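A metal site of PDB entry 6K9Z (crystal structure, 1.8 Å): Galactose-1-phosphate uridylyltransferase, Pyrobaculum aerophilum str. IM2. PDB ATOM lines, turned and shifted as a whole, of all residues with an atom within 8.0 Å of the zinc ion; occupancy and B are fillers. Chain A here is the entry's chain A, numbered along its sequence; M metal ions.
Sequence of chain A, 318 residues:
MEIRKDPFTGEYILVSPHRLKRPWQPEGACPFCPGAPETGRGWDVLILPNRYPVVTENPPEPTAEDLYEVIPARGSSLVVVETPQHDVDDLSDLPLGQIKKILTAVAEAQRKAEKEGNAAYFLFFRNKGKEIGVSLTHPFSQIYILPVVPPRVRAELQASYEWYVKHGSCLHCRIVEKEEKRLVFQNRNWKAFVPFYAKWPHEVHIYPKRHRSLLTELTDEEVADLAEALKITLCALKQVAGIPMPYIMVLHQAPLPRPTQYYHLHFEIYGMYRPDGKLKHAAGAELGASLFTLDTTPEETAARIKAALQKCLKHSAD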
ATOM      1  N   GLY A  28       7.620 -12.990  19.042  1.00  0.00           N
ATOM      2  CA  GLY A  28       8.234 -12.331  20.213  1.00  0.00           C
ATOM      3  C   GLY A  28       9.295 -11.303  19.841  1.00  0.00           C
ATOM      4  O   GLY A  28       9.747 -10.587  20.748  1.00  0.00           O
ATOM      5  N   ALA A  29       9.669 -11.203  18.563  1.00  0.00           N
ATOM      6  CA  ALA A  29      10.672 -10.202  18.129  1.00  0.00           C
ATOM      7  C   ALA A  29      10.058  -8.804  18.221  1.00  0.00           C
ATOM      8  O   ALA A  29       8.835  -8.699  17.998  1.00  0.00           O
ATOM      9  CB  ALA A  29      11.129 -10.503  16.725  1.00  0.00           C
ATOM     10  N   CYS A  30      10.847  -7.763  18.524  1.00  0.00           N
ATOM     11  CA  CYS A  30      10.215  -6.411  18.622  1.00  0.00           C
ATOM     12  C   CYS A  30      10.287  -5.728  17.261  1.00  0.00           C
ATOM     13  O   CYS A  30      11.387  -5.575  16.703  1.00  0.00           O
ATOM     14  CB  CYS A  30      10.905  -5.567  19.674  1.00  0.00           C
ATOM     15  SG  CYS A  30      10.229  -3.894  19.678  1.00  0.00           S
ATOM     16  N   PRO A  31       9.137  -5.290  16.677  1.00  0.00           N
ATOM     17  CA  PRO A  31       9.134  -4.652  15.341  1.00  0.00           C
ATOM     18  C   PRO A  31       9.774  -3.244  15.304  1.00  0.00           C
ATOM     19  O   PRO A  31      10.073  -2.711  14.180  1.00  0.00           O
ATOM     20  CB  PRO A  31       7.625  -4.579  14.993  1.00  0.00           C
ATOM     21  CG  PRO A  31       6.947  -4.437  16.335  1.00  0.00           C
ATOM     22  CD  PRO A  31       7.787  -5.321  17.275  1.00  0.00           C
ATOM     23  N   PHE A  32       9.968  -2.658  16.494  1.00  0.00           N
ATOM     24  CA  PHE A  32      10.351  -1.225  16.677  1.00  0.00           C
ATOM     25  C   PHE A  32      11.798  -1.078  17.152  1.00  0.00           C
ATOM     26  O   PHE A  32      12.306   0.016  17.031  1.00  0.00           O
ATOM     27  CB  PHE A  32       9.403  -0.522  17.652  1.00  0.00           C
ATOM     28  CG  PHE A  32       7.957  -0.545  17.234  1.00  0.00           C
ATOM     29  CD1 PHE A  32       7.610  -0.560  15.893  1.00  0.00           C
ATOM     30  CD2 PHE A  32       6.949  -0.530  18.200  1.00  0.00           C
ATOM     31  CE1 PHE A  32       6.268  -0.575  15.528  1.00  0.00           C
ATOM     32  CE2 PHE A  32       5.611  -0.547  17.826  1.00  0.00           C
ATOM     33  CZ  PHE A  32       5.276  -0.555  16.488  1.00  0.00           C
ATOM     34  N   CYS A  33      12.444  -2.143  17.600  1.00  0.00           N
ATOM     35  CA  CYS A  33      13.882  -2.127  17.916  1.00  0.00           C
ATOM     36  C   CYS A  33      14.727  -1.863  16.649  1.00  0.00           C
ATOM     37  O   CYS A  33      14.305  -2.111  15.484  1.00  0.00           O
ATOM     38  CB  CYS A  33      14.352  -3.416  18.561  1.00  0.00           C
ATOM     39  SG  CYS A  33      14.076  -3.447  20.355  1.00  0.00           S
ATOM     40  N   PRO A  34      15.908  -1.231  16.859  1.00  0.00           N
ATOM     41  CA  PRO A  34      16.876  -1.049  15.779  1.00  0.00           C
ATOM     42  C   PRO A  34      17.249  -2.443  15.247  1.00  0.00           C
ATOM     43  O   PRO A  34      17.357  -3.318  16.042  1.00  0.00           O
ATOM     44  CB  PRO A  34      18.076  -0.405  16.486  1.00  0.00           C
ATOM     45  CG  PRO A  34      17.468   0.317  17.657  1.00  0.00           C
ATOM     46  CD  PRO A  34      16.365  -0.620  18.121  1.00  0.00           C
ATOM     47  N   ALA A  36      15.217  -4.309  13.360  1.00  0.00           N
ATOM     48  CA  ALA A  36      13.940  -4.860  12.841  1.00  0.00           C
ATOM     49  C   ALA A  36      13.840  -4.469  11.351  1.00  0.00           C
ATOM     50  O   ALA A  36      14.609  -3.586  10.882  1.00  0.00           O
ATOM     51  CB  ALA A  36      12.769  -4.407  13.677  1.00  0.00           C
ATOM     52  N   THR A  39      12.926  -0.716  10.586  1.00  0.00           N
ATOM     53  CA  THR A  39      13.525   0.367  11.423  1.00  0.00           C
ATOM     54  C   THR A  39      14.947   0.789  11.031  1.00  0.00           C
ATOM     55  O   THR A  39      15.225   2.002  11.093  1.00  0.00           O
ATOM     56  CB  THR A  39      13.455   0.019  12.908  1.00  0.00           C
ATOM     57  OG1 THR A  39      14.243  -1.145  13.129  1.00  0.00           O
ATOM     58  CG2 THR A  39      12.036  -0.223  13.388  1.00  0.00           C
ATOM     59  N   TRP A  43      19.315   5.824  14.485  1.00  0.00           N
ATOM     60  CA  TRP A  43      18.239   6.845  14.616  1.00  0.00           C
ATOM     61  C   TRP A  43      17.906   7.093  16.087  1.00  0.00           C
ATOM     62  O   TRP A  43      18.038   6.167  16.894  1.00  0.00           O
ATOM     63  CB  TRP A  43      17.002   6.403  13.839  1.00  0.00           C
ATOM     64  CG  TRP A  43      16.561   5.010  14.136  1.00  0.00           C
ATOM     65  CD1 TRP A  43      16.922   3.873  13.452  1.00  0.00           C
ATOM     66  CD2 TRP A  43      15.686   4.573  15.190  1.00  0.00           C
ATOM     67  NE1 TRP A  43      16.331   2.781  14.007  1.00  0.00           N
ATOM     68  CE2 TRP A  43      15.558   3.168  15.075  1.00  0.00           C
ATOM     69  CE3 TRP A  43      14.993   5.226  16.209  1.00  0.00           C
ATOM     70  CZ2 TRP A  43      14.780   2.416  15.941  1.00  0.00           C
ATOM     71  CZ3 TRP A  43      14.215   4.475  17.075  1.00  0.00           C
ATOM     72  CH2 TRP A  43      14.109   3.090  16.931  1.00  0.00           C
ATOM     73  N   VAL A  81       8.314   5.762  16.862  1.00  0.00           N
ATOM     74  CA  VAL A  81       9.227   4.994  17.736  1.00  0.00           C
ATOM     75  C   VAL A  81      10.031   6.040  18.470  1.00  0.00           C
ATOM     76  O   VAL A  81      10.877   6.726  17.840  1.00  0.00           O
ATOM     77  CB  VAL A  81      10.070   3.966  16.982  1.00  0.00           C
ATOM     78  CG1 VAL A  81      10.787   3.035  17.950  1.00  0.00           C
ATOM     79  CG2 VAL A  81       9.268   3.190  15.964  1.00  0.00           C
ATOM     80  N   THR A  83      12.329   6.066  20.951  1.00  0.00           N
ATOM     81  CA  THR A  83      13.729   5.819  21.399  1.00  0.00           C
ATOM     82  C   THR A  83      14.155   4.504  20.791  1.00  0.00           C
ATOM     83  O   THR A  83      13.305   3.639  20.605  1.00  0.00           O
ATOM     84  CB  THR A  83      13.812   5.731  22.935  1.00  0.00           C
ATOM     85  OG1 THR A  83      15.115   5.299  23.314  1.00  0.00           O
ATOM     86  CG2 THR A  83      12.811   4.744  23.512  1.00  0.00           C
ATOM     87  N   PRO A  84      15.451   4.316  20.475  1.00  0.00           N
ATOM     88  CA  PRO A  84      15.955   3.012  20.064  1.00  0.00           C
ATOM     89  C   PRO A  84      15.998   1.997  21.238  1.00  0.00           C
ATOM     90  O   PRO A  84      16.044   0.833  20.987  1.00  0.00           O
ATOM     91  CB  PRO A  84      17.372   3.377  19.506  1.00  0.00           C
ATOM     92  CG  PRO A  84      17.765   4.663  20.191  1.00  0.00           C
ATOM     93  CD  PRO A  84      16.473   5.372  20.448  1.00  0.00           C
ATOM     94  N   GLN A  85      15.931   2.506  22.472  1.00  0.00           N
ATOM     95  CA  GLN A  85      16.026   1.636  23.685  1.00  0.00           C
ATOM     96  C   GLN A  85      14.668   1.008  24.003  1.00  0.00           C
ATOM     97  O   GLN A  85      13.701   1.751  24.244  1.00  0.00           O
ATOM     98  CB  GLN A  85      16.498   2.471  24.882  1.00  0.00           C
ATOM     99  CG  GLN A  85      17.954   2.901  24.793  1.00  0.00           C
ATOM    100  CD  GLN A  85      18.393   3.676  26.015  1.00  0.00           C
ATOM    101  OE1 GLN A  85      19.580   3.877  26.254  1.00  0.00           O
ATOM    102  NE2 GLN A  85      17.428   4.129  26.793  1.00  0.00           N
ATOM    103  N   HIS A  86      14.606  -0.329  23.965  1.00  0.00           N
ATOM    104  CA  HIS A  86      13.369  -1.091  24.258  1.00  0.00           C
ATOM    105  C   HIS A  86      12.981  -1.058  25.741  1.00  0.00           C
ATOM    106  O   HIS A  86      11.780  -0.920  26.021  1.00  0.00           O
ATOM    107  CB  HIS A  86      13.526  -2.547  23.786  1.00  0.00           C
ATOM    108  CG  HIS A  86      12.251  -3.312  23.807  1.00  0.00           C
ATOM    109  ND1 HIS A  86      11.515  -3.544  22.671  1.00  0.00           N
ATOM    110  CD2 HIS A  86      11.582  -3.897  24.820  1.00  0.00           C
ATOM    111  CE1 HIS A  86      10.443  -4.251  22.975  1.00  0.00           C
ATOM    112  NE2 HIS A  86      10.462  -4.477  24.297  1.00  0.00           N
ATOM    113  N   ASP A  87      13.953  -1.178  26.645  1.00  0.00           N
ATOM    114  CA  ASP A  87      13.637  -1.294  28.097  1.00  0.00           C
ATOM    115  C   ASP A  87      13.500   0.060  28.807  1.00  0.00           C
ATOM    116  O   ASP A  87      14.270   0.321  29.736  1.00  0.00           O
ATOM    117  CB  ASP A  87      14.598  -2.246  28.828  1.00  0.00           C
ATOM    118  CG  ASP A  87      13.940  -2.880  30.038  1.00  0.00           C
ATOM    119  OD1 ASP A  87      12.787  -3.342  29.906  1.00  0.00           O
ATOM    120  OD2 ASP A  87      14.588  -2.912  31.106  1.00  0.00           O
ATOM    121  N   LEU A 136       2.706  -4.366  22.961  1.00  0.00           N
ATOM    122  CA  LEU A 136       4.128  -4.104  22.578  1.00  0.00           C
ATOM    123  C   LEU A 136       4.768  -3.216  23.665  1.00  0.00           C
ATOM    124  O   LEU A 136       4.193  -2.193  24.008  1.00  0.00           O
ATOM    125  CB  LEU A 136       4.174  -3.412  21.204  1.00  0.00           C
ATOM    126  CG  LEU A 136       3.722  -4.234  20.001  1.00  0.00           C
ATOM    127  CD1 LEU A 136       3.523  -3.322  18.811  1.00  0.00           C
ATOM    128  CD2 LEU A 136       4.722  -5.336  19.646  1.00  0.00           C
ATOM    129  N   THR A 137       5.951  -3.578  24.164  1.00  0.00           N
ATOM    130  CA  THR A 137       6.583  -2.934  25.357  1.00  0.00           C
ATOM    131  C   THR A 137       7.526  -1.792  24.927  1.00  0.00           C
ATOM    132  O   THR A 137       7.851  -0.906  25.757  1.00  0.00           O
ATOM    133  CB  THR A 137       7.214  -4.024  26.230  1.00  0.00           C
ATOM    134  OG1 THR A 137       8.071  -4.905  25.499  1.00  0.00           O
ATOM    135  CG2 THR A 137       6.131  -4.864  26.879  1.00  0.00           C
ATOM    136  N   HIS A 138       7.898  -1.722  23.656  1.00  0.00           N
ATOM    137  CA  HIS A 138       8.790  -0.633  23.151  1.00  0.00           C
ATOM    138  C   HIS A 138       8.020   0.673  23.213  1.00  0.00           C
ATOM    139  O   HIS A 138       6.870   0.697  22.796  1.00  0.00           O
ATOM    140  CB  HIS A 138       9.265  -0.973  21.732  1.00  0.00           C
ATOM    141  CG  HIS A 138      10.503  -0.233  21.333  1.00  0.00           C
ATOM    142  ND1 HIS A 138      11.698  -0.834  21.129  1.00  0.00           N
ATOM    143  CD2 HIS A 138      10.690   1.084  21.116  1.00  0.00           C
ATOM    144  CE1 HIS A 138      12.607   0.059  20.762  1.00  0.00           C
ATOM    145  NE2 HIS A 138      12.007   1.284  20.783  1.00  0.00           N
ATOM    146  N   PRO A 139       8.629   1.765  23.762  1.00  0.00           N
ATOM    147  CA  PRO A 139       7.983   3.067  23.833  1.00  0.00           C
ATOM    148  C   PRO A 139       7.640   3.560  22.425  1.00  0.00           C
ATOM    149  O   PRO A 139       8.524   3.681  21.582  1.00  0.00           O
ATOM    150  CB  PRO A 139       9.032   4.005  24.431  1.00  0.00           C
ATOM    151  CG  PRO A 139       9.880   3.082  25.239  1.00  0.00           C
ATOM    152  CD  PRO A 139       9.961   1.823  24.402  1.00  0.00           C
HETATM  153 ZN    ZN M   1      11.901  -2.930  20.881  1.00  0.00          ZN
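The side-chain hydroxyl (OG1) of Thr 137 lies within hydrogen-bond range of a ring nitrogen (NE2) of His 86 (2.7 Å).
NE2 of His 138 lies within hydrogen-bond range of O of Thr 83 (2.7 Å).
The side-chain sulfur (SG) of Cys 30 sits close to the backbone NH (N) of Phe 32, 3.4 Å away.
The backbone carbonyl oxygen (O) of Cys 33 sits at hydrogen-bond distance from the side-chain hydroxyl (OG1) of Thr 39 (2.5 Å).
Four residues have an atom within 4 Å of the zinc ion: Cys 30, Cys 33, His 86 and His 138.
The zinc ion is bound by a ring nitrogen (ND1) of His 86, 1.9 Å away.
The zinc ion is bound by ND1 of His 138, 2.1 Å away.
The zinc ion is bound by SG of Cys 30, at 2.3 Å.
The zinc ion is bound by SG of Cys 33 (2.3 Å).
The zinc ion has four donor atoms within binding distance.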
